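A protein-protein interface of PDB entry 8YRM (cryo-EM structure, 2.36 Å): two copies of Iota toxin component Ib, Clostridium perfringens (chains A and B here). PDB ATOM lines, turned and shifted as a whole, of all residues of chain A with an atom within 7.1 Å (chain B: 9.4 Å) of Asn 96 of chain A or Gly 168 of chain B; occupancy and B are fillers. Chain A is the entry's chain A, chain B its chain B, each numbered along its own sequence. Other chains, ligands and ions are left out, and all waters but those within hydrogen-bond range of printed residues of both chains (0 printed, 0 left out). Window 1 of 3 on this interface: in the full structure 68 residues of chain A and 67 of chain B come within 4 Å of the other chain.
Of the printed residues of chain B, Ser 94 of chain A touches Asn 247 (2.8 Å). Printed residues of chain B within 4 Å of Thr 95 of chain A: Lys 167 (3.4 Å) and Gly 168 (3.3 Å). Asn 96 of chain A touches just these residues of chain B: Asn 166 (3.7 Å) and Gly 168 (3.8 Å). No residue of chain B comes within 4 Å of Ala 171 of chain A. Pro 245 of chain A touches none of the printed residues of chain B. Printed residues of chain A within 4 Å of Ile 165 of chain B: Glu 97 and His 98. Printed residues of chain A within 4 Å of Asn 166 of chain B: Asn 96 (3.7 Å), Glu 97 (3.6 Å) and His 98 (3.9 Å). Gly 168 of chain B touches just these residues of chain A: Thr 95 and Asn 96. Of the printed residues of chain A, Glu 169 of chain B touches Leu 243. The nearest printed residue of chain B that does not touch Ser 94 of chain A is Gly 168 of chain B (4.1 Å).
The side-chain amide nitrogen of Asn 96 of chain A sits at hydrogen-bond distance from the backbone carbonyl oxygen of Glu 169 of chain A, 2.7 Å away. O of Ser 164 of chain A is in hydrogen-bond range of N of His 98 of chain A, at 2.8 Å. The side-chain hydroxyl of Ser 170 of chain B is in hydrogen-bond range of the backbone carbonyl oxygen of Asn 166 of chain B (2.8 Å). The side-chain carboxylate of Glu 169 of chain B is in hydrogen-bond range of the side-chain hydroxyl of Tyr 172 of chain B. The side-chain carboxylate of Glu 169 of chain B lies within salt-bridge range of the guanidinium group of Arg 242 of chain B. N of Asn 247 of chain B is in hydrogen-bond range of OE1 of Gln 250 of chain B (2.9 Å).
ND2 of Asn 247 of chain B touches O of Ile 93 of chain A (3.96 Å). C of Lys 167 of chain B touches O of Thr 95 of chain A, at 3.4 Å. OD1 of Asn 166 of chain B touches CA of Asn 96 of chain A, at 3.7 Å. CA of Asn 96 of chain A touches N of Gly 168 of chain B, at 3.8 Å. Ile 165 of chain B touches Glu 97 of chain A. O of Glu 97 of chain A touches OD1 of Asn 166 of chain B (3.6 Å). His 98 of chain A touches Ile 165 of chain B. His 98 of chain A touches Asn 166 of chain B (ND1 to N, 3.9 Å). Leu 243 of chain A touches Glu 169 of chain B. CD1 of Leu 243 of chain A touches NH2 of Arg 242 of chain B (3.5 Å).
Of the 17 printed residues of chain A, 7 touch a printed residue of chain B. Printed residues of chain A that touch a printed residue of chain B: Ile 93, Ser 94, Thr 95, Asn 96, Glu 97, His 98 and Leu 243. Among the printed residues, no Asp or Glu carboxylate lies within 4 Å of a Lys or Arg side-chain nitrogen of the other chain.
Asn 96 of chain A touches Asn 166 of chain B, but with the chains exchanged Asn 166 of chain A does not touch Asn 96 of chain B (15.2 Å). 10 positions are printed for both chains. Of the 13 pairs that touch across the chains among the printed residues, none has its exchanged pair printed and touching as well.
ND2 of Asn 247 of chain B is in hydrogen-bond range of OG of Ser 94 of chain A (2.8 Å). The backbone carbonyl oxygen (O) of Thr 95 of chain A sits at hydrogen-bond distance from the backbone NH (N) of Gly 168 of chain B. The backbone NH of Lys 167 of chain B is in hydrogen-bond range of the backbone carbonyl oxygen of Glu 97 of chain A (3.0 Å).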
ATOM      1  N   ILE A  93      -2.656  13.690   1.334  1.00  0.00           N
ATOM      2  CA  ILE A  93      -4.037  13.715   1.784  1.00  0.00           C
ATOM      3  C   ILE A  93      -4.845  12.723   0.952  1.00  0.00           C
ATOM      4  O   ILE A  93      -4.833  12.780  -0.272  1.00  0.00           O
ATOM      5  CB  ILE A  93      -4.620  15.136   1.668  1.00  0.00           C
ATOM      6  CG1 ILE A  93      -3.788  16.145   2.435  1.00  0.00           C
ATOM      7  CG2 ILE A  93      -6.070  15.170   2.139  1.00  0.00           C
ATOM      8  CD1 ILE A  93      -3.877  17.548   1.875  1.00  0.00           C
ATOM      9  N   SER A  94      -5.572  11.839   1.632  1.00  0.00           N
ATOM     10  CA  SER A  94      -6.456  10.888   0.985  1.00  0.00           C
ATOM     11  C   SER A  94      -7.885  11.219   1.379  1.00  0.00           C
ATOM     12  O   SER A  94      -8.292  10.938   2.503  1.00  0.00           O
ATOM     13  CB  SER A  94      -6.110   9.463   1.368  1.00  0.00           C
ATOM     14  OG  SER A  94      -4.742   9.168   1.122  1.00  0.00           O
ATOM     15  N   THR A  95      -8.639  11.818   0.453  1.00  0.00           N
ATOM     16  CA  THR A  95     -10.014  12.205   0.719  1.00  0.00           C
ATOM     17  C   THR A  95     -10.893  10.969   0.639  1.00  0.00           C
ATOM     18  O   THR A  95     -11.017  10.379  -0.428  1.00  0.00           O
ATOM     19  CB  THR A  95     -10.478  13.249  -0.294  1.00  0.00           C
ATOM     20  OG1 THR A  95      -9.492  14.275  -0.285  1.00  0.00           O
ATOM     21  CG2 THR A  95     -11.831  13.820   0.081  1.00  0.00           C
ATOM     22  N   ASN A  96     -11.517  10.588   1.752  1.00  0.00           N
ATOM     23  CA  ASN A  96     -12.333   9.390   1.726  1.00  0.00           C
ATOM     24  C   ASN A  96     -13.774   9.786   1.444  1.00  0.00           C
ATOM     25  O   ASN A  96     -14.612   9.787   2.329  1.00  0.00           O
ATOM     26  CB  ASN A  96     -12.144   8.494   2.944  1.00  0.00           C
ATOM     27  CG  ASN A  96     -12.388   9.227   4.228  1.00  0.00           C
ATOM     28  OD1 ASN A  96     -11.476   9.879   4.747  1.00  0.00           O
ATOM     29  ND2 ASN A  96     -13.584   9.083   4.773  1.00  0.00           N
ATOM     30  N   GLU A  97     -14.038  10.059   0.168  1.00  0.00           N
ATOM     31  CA  GLU A  97     -15.385  10.263  -0.328  1.00  0.00           C
ATOM     32  C   GLU A  97     -15.802   9.061  -1.168  1.00  0.00           C
ATOM     33  O   GLU A  97     -14.996   8.501  -1.905  1.00  0.00           O
ATOM     34  CB  GLU A  97     -15.467  11.565  -1.116  1.00  0.00           C
ATOM     35  CG  GLU A  97     -14.496  11.659  -2.283  1.00  0.00           C
ATOM     36  CD  GLU A  97     -14.331  13.083  -2.789  1.00  0.00           C
ATOM     37  OE1 GLU A  97     -15.045  13.980  -2.282  1.00  0.00           O
ATOM     38  OE2 GLU A  97     -13.478  13.303  -3.683  1.00  0.00           O
ATOM     39  N   HIS A  98     -17.069   8.667  -1.026  1.00  0.00           N
ATOM     40  CA  HIS A  98     -17.600   7.529  -1.745  1.00  0.00           C
ATOM     41  C   HIS A  98     -18.236   8.035  -3.035  1.00  0.00           C
ATOM     42  O   HIS A  98     -19.189   8.797  -2.985  1.00  0.00           O
ATOM     43  CB  HIS A  98     -18.549   6.736  -0.849  1.00  0.00           C
ATOM     44  CG  HIS A  98     -18.901   5.392  -1.414  1.00  0.00           C
ATOM     45  ND1 HIS A  98     -18.020   4.330  -1.413  1.00  0.00           N
ATOM     46  CD2 HIS A  98     -20.021   4.939  -2.003  1.00  0.00           C
ATOM     47  CE1 HIS A  98     -18.599   3.276  -1.973  1.00  0.00           C
ATOM     48  NE2 HIS A  98     -19.817   3.623  -2.334  1.00  0.00           N
ATOM     49  N   SER A 164     -20.695  10.888  -1.794  1.00  0.00           N
ATOM     50  CA  SER A 164     -21.010  11.132  -0.400  1.00  0.00           C
ATOM     51  C   SER A 164     -19.723  11.251   0.411  1.00  0.00           C
ATOM     52  O   SER A 164     -18.700  10.665   0.058  1.00  0.00           O
ATOM     53  CB  SER A 164     -21.890  10.048   0.131  1.00  0.00           C
ATOM     54  OG  SER A 164     -21.154   8.848   0.325  1.00  0.00           O
ATOM     55  N   ILE A 165     -19.789  12.019   1.499  1.00  0.00           N
ATOM     56  CA  ILE A 165     -18.643  12.260   2.353  1.00  0.00           C
ATOM     57  C   ILE A 165     -19.115  12.257   3.801  1.00  0.00           C
ATOM     58  O   ILE A 165     -20.201  12.731   4.105  1.00  0.00           O
ATOM     59  CB  ILE A 165     -17.944  13.584   1.990  1.00  0.00           C
ATOM     60  CG1 ILE A 165     -16.663  13.804   2.806  1.00  0.00           C
ATOM     61  CG2 ILE A 165     -18.891  14.770   2.144  1.00  0.00           C
ATOM     62  CD1 ILE A 165     -15.422  13.140   2.244  1.00  0.00           C
ATOM     63  N   ASN A 166     -18.288  11.696   4.680  1.00  0.00           N
ATOM     64  CA  ASN A 166     -18.443  11.835   6.116  1.00  0.00           C
ATOM     65  C   ASN A 166     -17.712  13.095   6.571  1.00  0.00           C
ATOM     66  O   ASN A 166     -16.546  13.302   6.240  1.00  0.00           O
ATOM     67  CB  ASN A 166     -17.882  10.615   6.831  1.00  0.00           C
ATOM     68  CG  ASN A 166     -18.068  10.672   8.328  1.00  0.00           C
ATOM     69  OD1 ASN A 166     -18.887  11.440   8.847  1.00  0.00           O
ATOM     70  ND2 ASN A 166     -17.332   9.838   9.044  1.00  0.00           N
ATOM     71  N   GLU A 169     -14.785  12.385   9.417  1.00  0.00           N
ATOM     72  CA  GLU A 169     -13.592  11.723   8.919  1.00  0.00           C
ATOM     73  C   GLU A 169     -13.525  11.926   7.411  1.00  0.00           C
ATOM     74  O   GLU A 169     -13.693  10.995   6.635  1.00  0.00           O
ATOM     75  CB  GLU A 169     -13.617  10.237   9.255  1.00  0.00           C
ATOM     76  CG  GLU A 169     -13.380   9.945  10.734  1.00  0.00           C
ATOM     77  CD  GLU A 169     -12.739   8.587  11.001  1.00  0.00           C
ATOM     78  OE1 GLU A 169     -12.334   7.883  10.043  1.00  0.00           O
ATOM     79  OE2 GLU A 169     -12.648   8.229  12.195  1.00  0.00           O
ATOM     80  N   SER A 170     -13.297  13.169   7.013  1.00  0.00           N
ATOM     81  CA  SER A 170     -13.343  13.523   5.612  1.00  0.00           C
ATOM     82  C   SER A 170     -12.131  12.981   4.860  1.00  0.00           C
ATOM     83  O   SER A 170     -12.259  12.549   3.720  1.00  0.00           O
ATOM     84  CB  SER A 170     -13.484  14.997   5.477  1.00  0.00           C
ATOM     85  OG  SER A 170     -14.679  15.395   6.130  1.00  0.00           O
ATOM     86  N   ALA A 171     -10.964  12.999   5.494  1.00  0.00           N
ATOM     87  CA  ALA A 171      -9.733  12.642   4.813  1.00  0.00           C
ATOM     88  C   ALA A 171      -8.782  11.974   5.793  1.00  0.00           C
ATOM     89  O   ALA A 171      -8.972  12.068   7.003  1.00  0.00           O
ATOM     90  CB  ALA A 171      -9.105  13.865   4.204  1.00  0.00           C
ATOM     91  N   TYR A 172      -7.781  11.282   5.243  1.00  0.00           N
ATOM     92  CA  TYR A 172      -6.683  10.734   6.022  1.00  0.00           C
ATOM     93  C   TYR A 172      -5.384  11.366   5.556  1.00  0.00           C
ATOM     94  O   TYR A 172      -5.231  11.644   4.371  1.00  0.00           O
ATOM     95  CB  TYR A 172      -6.577   9.222   5.854  1.00  0.00           C
ATOM     96  CG  TYR A 172      -7.808   8.494   6.351  1.00  0.00           C
ATOM     97  CD1 TYR A 172      -8.182   8.570   7.687  1.00  0.00           C
ATOM     98  CD2 TYR A 172      -8.592   7.738   5.495  1.00  0.00           C
ATOM     99  CE1 TYR A 172      -9.314   7.922   8.155  1.00  0.00           C
ATOM    100  CE2 TYR A 172      -9.726   7.089   5.947  1.00  0.00           C
ATOM    101  CZ  TYR A 172     -10.089   7.180   7.279  1.00  0.00           C
ATOM    102  OH  TYR A 172     -11.202   6.522   7.721  1.00  0.00           O
ATOM    103  N   LEU A 243      -5.889   4.762  10.534  1.00  0.00           N
ATOM    104  CA  LEU A 243      -5.371   5.927   9.832  1.00  0.00           C
ATOM    105  C   LEU A 243      -5.700   7.212  10.590  1.00  0.00           C
ATOM    106  O   LEU A 243      -6.593   7.225  11.430  1.00  0.00           O
ATOM    107  CB  LEU A 243      -5.955   5.965   8.425  1.00  0.00           C
ATOM    108  CG  LEU A 243      -5.687   4.728   7.557  1.00  0.00           C
ATOM    109  CD1 LEU A 243      -6.381   4.871   6.232  1.00  0.00           C
ATOM    110  CD2 LEU A 243      -4.221   4.473   7.308  1.00  0.00           C
ATOM    111  N   PRO A 245      -7.295  10.663  10.928  1.00  0.00           N
ATOM    112  CA  PRO A 245      -8.382  11.413  10.292  1.00  0.00           C
ATOM    113  C   PRO A 245      -8.304  12.917  10.479  1.00  0.00           C
ATOM    114  O   PRO A 245      -7.744  13.382  11.461  1.00  0.00           O
ATOM    115  CB  PRO A 245      -9.603  10.824  10.978  1.00  0.00           C
ATOM    116  CG  PRO A 245      -9.133  10.488  12.378  1.00  0.00           C
ATOM    117  CD  PRO A 245      -7.643  10.219  12.285  1.00  0.00           C
ATOM    118  N   ILE A 246      -8.871  13.655   9.523  1.00  0.00           N
ATOM    119  CA  ILE A 246      -9.185  15.065   9.697  1.00  0.00           C
ATOM    120  C   ILE A 246     -10.642  15.294   9.308  1.00  0.00           C
ATOM    121  O   ILE A 246     -11.203  14.505   8.550  1.00  0.00           O
ATOM    122  CB  ILE A 246      -8.232  15.937   8.874  1.00  0.00           C
ATOM    123  CG1 ILE A 246      -8.346  15.639   7.391  1.00  0.00           C
ATOM    124  CG2 ILE A 246      -6.796  15.774   9.381  1.00  0.00           C
ATOM    125  CD1 ILE A 246      -7.625  16.650   6.519  1.00  0.00           C
ATOM    126  N   LEU A 251     -10.100  19.809   6.218  1.00  0.00           N
ATOM    127  CA  LEU A 251      -9.830  19.453   4.835  1.00  0.00           C
ATOM    128  C   LEU A 251      -9.985  20.684   3.945  1.00  0.00           C
ATOM    129  O   LEU A 251      -9.192  20.893   3.032  1.00  0.00           O
ATOM    130  CB  LEU A 251     -10.740  18.317   4.380  1.00  0.00           C
ATOM    131  CG  LEU A 251     -10.628  17.912   2.905  1.00  0.00           C
ATOM    132  CD1 LEU A 251      -9.261  17.369   2.554  1.00  0.00           C
ATOM    133  CD2 LEU A 251     -11.677  16.878   2.583  1.00  0.00           C
ATOM    134  N   ASN B  96     -10.498  -2.170  -4.900  1.00  0.00           N
ATOM    135  CA  ASN B  96     -11.683  -2.499  -4.131  1.00  0.00           C
ATOM    136  C   ASN B  96     -12.808  -1.563  -4.541  1.00  0.00           C
ATOM    137  O   ASN B  96     -13.155  -0.642  -3.822  1.00  0.00           O
ATOM    138  CB  ASN B  96     -11.435  -2.579  -2.629  1.00  0.00           C
ATOM    139  CG  ASN B  96     -10.832  -1.320  -2.087  1.00  0.00           C
ATOM    140  OD1 ASN B  96      -9.609  -1.152  -2.132  1.00  0.00           O
ATOM    141  ND2 ASN B  96     -11.666  -0.458  -1.526  1.00  0.00           N
ATOM    142  N   ILE B 165     -16.788   3.346  -5.664  1.00  0.00           N
ATOM    143  CA  ILE B 165     -15.416   3.279  -5.200  1.00  0.00           C
ATOM    144  C   ILE B 165     -15.248   4.270  -4.056  1.00  0.00           C
ATOM    145  O   ILE B 165     -15.824   5.349  -4.075  1.00  0.00           O
ATOM    146  CB  ILE B 165     -14.425   3.564  -6.345  1.00  0.00           C
ATOM    147  CG1 ILE B 165     -12.968   3.386  -5.904  1.00  0.00           C
ATOM    148  CG2 ILE B 165     -14.644   4.955  -6.934  1.00  0.00           C
ATOM    149  CD1 ILE B 165     -12.444   1.964  -5.972  1.00  0.00           C
ATOM    150  N   ASN B 166     -14.464   3.874  -3.055  1.00  0.00           N
ATOM    151  CA  ASN B 166     -13.978   4.774  -2.026  1.00  0.00           C
ATOM    152  C   ASN B 166     -12.673   5.408  -2.499  1.00  0.00           C
ATOM    153  O   ASN B 166     -11.757   4.714  -2.934  1.00  0.00           O
ATOM    154  CB  ASN B 166     -13.756   4.020  -0.723  1.00  0.00           C
ATOM    155  CG  ASN B 166     -13.307   4.916   0.406  1.00  0.00           C
ATOM    156  OD1 ASN B 166     -13.460   6.142   0.355  1.00  0.00           O
ATOM    157  ND2 ASN B 166     -12.778   4.315   1.460  1.00  0.00           N
ATOM    158  N   LYS B 167     -12.584   6.734  -2.415  1.00  0.00           N
ATOM    159  CA  LYS B 167     -11.451   7.435  -2.995  1.00  0.00           C
ATOM    160  C   LYS B 167     -10.262   7.515  -2.040  1.00  0.00           C
ATOM    161  O   LYS B 167      -9.180   7.919  -2.459  1.00  0.00           O
ATOM    162  CB  LYS B 167     -11.870   8.820  -3.482  1.00  0.00           C
ATOM    163  CG  LYS B 167     -12.809   8.732  -4.659  1.00  0.00           C
ATOM    164  CD  LYS B 167     -12.776   9.950  -5.564  1.00  0.00           C
ATOM    165  CE  LYS B 167     -13.252   9.609  -6.936  1.00  0.00           C
ATOM    166  NZ  LYS B 167     -13.346  10.815  -7.761  1.00  0.00           N
ATOM    167  N   GLY B 168     -10.460   7.146  -0.771  1.00  0.00           N
ATOM    168  CA  GLY B 168      -9.370   7.136   0.191  1.00  0.00           C
ATOM    169  C   GLY B 168      -8.695   5.771   0.261  1.00  0.00           C
ATOM    170  O   GLY B 168      -7.504   5.693   0.538  1.00  0.00           O
ATOM    171  N   GLU B 169      -9.472   4.706   0.035  1.00  0.00           N
ATOM    172  CA  GLU B 169      -8.963   3.348   0.019  1.00  0.00           C
ATOM    173  C   GLU B 169      -9.404   2.684  -1.280  1.00  0.00           C
ATOM    174  O   GLU B 169     -10.233   1.784  -1.286  1.00  0.00           O
ATOM    175  CB  GLU B 169      -9.480   2.560   1.217  1.00  0.00           C
ATOM    176  CG  GLU B 169      -8.837   2.976   2.537  1.00  0.00           C
ATOM    177  CD  GLU B 169      -8.779   1.860   3.576  1.00  0.00           C
ATOM    178  OE1 GLU B 169      -9.112   0.690   3.261  1.00  0.00           O
ATOM    179  OE2 GLU B 169      -8.397   2.172   4.723  1.00  0.00           O
ATOM    180  N   SER B 170      -8.848   3.164  -2.383  1.00  0.00           N
ATOM    181  CA  SER B 170      -9.276   2.718  -3.689  1.00  0.00           C
ATOM    182  C   SER B 170      -8.799   1.298  -3.977  1.00  0.00           C
ATOM    183  O   SER B 170      -9.525   0.518  -4.583  1.00  0.00           O
ATOM    184  CB  SER B 170      -8.824   3.690  -4.720  1.00  0.00           C
ATOM    185  OG  SER B 170      -9.387   4.958  -4.417  1.00  0.00           O
ATOM    186  N   ALA B 171      -7.590   0.962  -3.544  1.00  0.00           N
ATOM    187  CA  ALA B 171      -6.991  -0.312  -3.896  1.00  0.00           C
ATOM    188  C   ALA B 171      -6.115  -0.798  -2.753  1.00  0.00           C
ATOM    189  O   ALA B 171      -5.762  -0.021  -1.869  1.00  0.00           O
ATOM    190  CB  ALA B 171      -6.195  -0.178  -5.167  1.00  0.00           C
ATOM    191  N   TYR B 172      -5.794  -2.093  -2.785  1.00  0.00           N
ATOM    192  CA  TYR B 172      -4.823  -2.685  -1.880  1.00  0.00           C
ATOM    193  C   TYR B 172      -3.670  -3.246  -2.690  1.00  0.00           C
ATOM    194  O   TYR B 172      -3.885  -3.748  -3.790  1.00  0.00           O
ATOM    195  CB  TYR B 172      -5.436  -3.815  -1.059  1.00  0.00           C
ATOM    196  CG  TYR B 172      -6.559  -3.339  -0.163  1.00  0.00           C
ATOM    197  CD1 TYR B 172      -6.321  -2.408   0.838  1.00  0.00           C
ATOM    198  CD2 TYR B 172      -7.852  -3.816  -0.318  1.00  0.00           C
ATOM    199  CE1 TYR B 172      -7.343  -1.951   1.654  1.00  0.00           C
ATOM    200  CE2 TYR B 172      -8.884  -3.366   0.487  1.00  0.00           C
ATOM    201  CZ  TYR B 172      -8.630  -2.433   1.476  1.00  0.00           C
ATOM    202  OH  TYR B 172      -9.650  -2.006   2.278  1.00  0.00           O
ATOM    203  N   ARG B 242      -4.673  -6.185   8.468  1.00  0.00           N
ATOM    204  CA  ARG B 242      -5.062  -4.967   7.779  1.00  0.00           C
ATOM    205  C   ARG B 242      -4.246  -4.839   6.495  1.00  0.00           C
ATOM    206  O   ARG B 242      -3.022  -4.778   6.548  1.00  0.00           O
ATOM    207  CB  ARG B 242      -4.848  -3.793   8.738  1.00  0.00           C
ATOM    208  CG  ARG B 242      -4.840  -2.396   8.134  1.00  0.00           C
ATOM    209  CD  ARG B 242      -6.229  -1.941   7.888  1.00  0.00           C
ATOM    210  NE  ARG B 242      -6.279  -0.479   7.782  1.00  0.00           N
ATOM    211  CZ  ARG B 242      -6.641   0.199   6.709  1.00  0.00           C
ATOM    212  NH1 ARG B 242      -6.663  -0.374   5.512  1.00  0.00           N
ATOM    213  NH2 ARG B 242      -6.940   1.478   6.843  1.00  0.00           N
ATOM    214  N   ILE B 244      -2.804  -3.127   2.884  1.00  0.00           N
ATOM    215  CA  ILE B 244      -2.081  -1.893   2.613  1.00  0.00           C
ATOM    216  C   ILE B 244      -2.871  -1.074   1.603  1.00  0.00           C
ATOM    217  O   ILE B 244      -2.957  -1.467   0.447  1.00  0.00           O
ATOM    218  CB  ILE B 244      -0.673  -2.208   2.078  1.00  0.00           C
ATOM    219  CG1 ILE B 244       0.054  -3.169   3.000  1.00  0.00           C
ATOM    220  CG2 ILE B 244       0.132  -0.927   1.841  1.00  0.00           C
ATOM    221  CD1 ILE B 244       1.253  -3.827   2.357  1.00  0.00           C
ATOM    222  N   PRO B 245      -3.463   0.078   1.989  1.00  0.00           N
ATOM    223  CA  PRO B 245      -4.285   0.866   1.066  1.00  0.00           C
ATOM    224  C   PRO B 245      -3.516   1.895   0.260  1.00  0.00           C
ATOM    225  O   PRO B 245      -2.483   2.373   0.704  1.00  0.00           O
ATOM    226  CB  PRO B 245      -5.272   1.520   2.020  1.00  0.00           C
ATOM    227  CG  PRO B 245      -4.488   1.737   3.298  1.00  0.00           C
ATOM    228  CD  PRO B 245      -3.413   0.668   3.335  1.00  0.00           C
ATOM    229  N   ILE B 246      -4.042   2.221  -0.924  1.00  0.00           N
ATOM    230  CA  ILE B 246      -3.638   3.404  -1.667  1.00  0.00           C
ATOM    231  C   ILE B 246      -4.888   4.188  -2.054  1.00  0.00           C
ATOM    232  O   ILE B 246      -5.974   3.613  -2.120  1.00  0.00           O
ATOM    233  CB  ILE B 246      -2.805   3.018  -2.892  1.00  0.00           C
ATOM    234  CG1 ILE B 246      -3.598   2.144  -3.848  1.00  0.00           C
ATOM    235  CG2 ILE B 246      -1.500   2.348  -2.454  1.00  0.00           C
ATOM    236  CD1 ILE B 246      -2.917   1.957  -5.191  1.00  0.00           C
ATOM    237  N   ASN B 247      -4.725   5.500  -2.298  1.00  0.00           N
ATOM    238  CA  ASN B 247      -5.857   6.362  -2.598  1.00  0.00           C
ATOM    239  C   ASN B 247      -6.081   6.382  -4.105  1.00  0.00           C
ATOM    240  O   ASN B 247      -5.356   5.728  -4.846  1.00  0.00           O
ATOM    241  CB  ASN B 247      -5.718   7.750  -1.981  1.00  0.00           C
ATOM    242  CG  ASN B 247      -4.524   8.519  -2.481  1.00  0.00           C
ATOM    243  OD1 ASN B 247      -4.225   8.504  -3.679  1.00  0.00           O
ATOM    244  ND2 ASN B 247      -3.823   9.178  -1.567  1.00  0.00           N
ATOM    245  N   TYR B 248      -7.083   7.146  -4.539  1.00  0.00           N
ATOM    246  CA  TYR B 248      -7.507   7.155  -5.923  1.00  0.00           C
ATOM    247  C   TYR B 248      -6.428   7.763  -6.813  1.00  0.00           C
ATOM    248  O   TYR B 248      -6.209   7.274  -7.916  1.00  0.00           O
ATOM    249  CB  TYR B 248      -8.841   7.899  -6.040  1.00  0.00           C
ATOM    250  CG  TYR B 248      -9.509   7.680  -7.388  1.00  0.00           C
ATOM    251  CD1 TYR B 248      -9.998   6.427  -7.733  1.00  0.00           C
ATOM    252  CD2 TYR B 248      -9.629   8.709  -8.318  1.00  0.00           C
ATOM    253  CE1 TYR B 248     -10.590   6.201  -8.966  1.00  0.00           C
ATOM    254  CE2 TYR B 248     -10.229   8.498  -9.549  1.00  0.00           C
ATOM    255  CZ  TYR B 248     -10.710   7.241  -9.873  1.00  0.00           C
ATOM    256  OH  TYR B 248     -11.304   7.017 -11.084  1.00  0.00           O
ATOM    257  N   ASP B 249      -5.760   8.820  -6.342  1.00  0.00           N
ATOM    258  CA  ASP B 249      -4.753   9.487  -7.150  1.00  0.00           C
ATOM    259  C   ASP B 249      -3.576   8.553  -7.392  1.00  0.00           C
ATOM    260  O   ASP B 249      -3.040   8.498  -8.497  1.00  0.00           O
ATOM    261  CB  ASP B 249      -4.312  10.802  -6.535  1.00  0.00           C
ATOM    262  CG  ASP B 249      -5.442  11.799  -6.321  1.00  0.00           C
ATOM    263  OD1 ASP B 249      -6.194  12.058  -7.295  1.00  0.00           O
ATOM    264  OD2 ASP B 249      -5.570  12.306  -5.182  1.00  0.00           O
ATOM    265  N   GLN B 250      -3.182   7.824  -6.348  1.00  0.00           N
ATOM    266  CA  GLN B 250      -2.093   6.874  -6.459  1.00  0.00           C
ATOM    267  C   GLN B 250      -2.479   5.732  -7.398  1.00  0.00           C
ATOM    268  O   GLN B 250      -1.653   5.263  -8.171  1.00  0.00           O
ATOM    269  CB  GLN B 250      -1.752   6.398  -5.049  1.00  0.00           C
ATOM    270  CG  GLN B 250      -1.044   7.465  -4.228  1.00  0.00           C
ATOM    271  CD  GLN B 250      -1.245   7.337  -2.736  1.00  0.00           C
ATOM    272  OE1 GLN B 250      -1.986   6.485  -2.233  1.00  0.00           O
ATOM    273  NE2 GLN B 250      -0.553   8.194  -2.006  1.00  0.00           N
ATOM    274  N   LEU B 251      -3.734   5.275  -7.320  1.00  0.00           N
ATOM    275  CA  LEU B 251      -4.195   4.196  -8.177  1.00  0.00           C
ATOM    276  C   LEU B 251      -4.149   4.641  -9.638  1.00  0.00           C
ATOM    277  O   LEU B 251      -3.760   3.869 -10.509  1.00  0.00           O
ATOM    278  CB  LEU B 251      -5.594   3.745  -7.777  1.00  0.00           C
ATOM    279  CG  LEU B 251      -6.240   2.677  -8.666  1.00  0.00           C
ATOM    280  CD1 LEU B 251      -5.483   1.370  -8.650  1.00  0.00           C
ATOM    281  CD2 LEU B 251      -7.661   2.437  -8.220  1.00  0.00           C
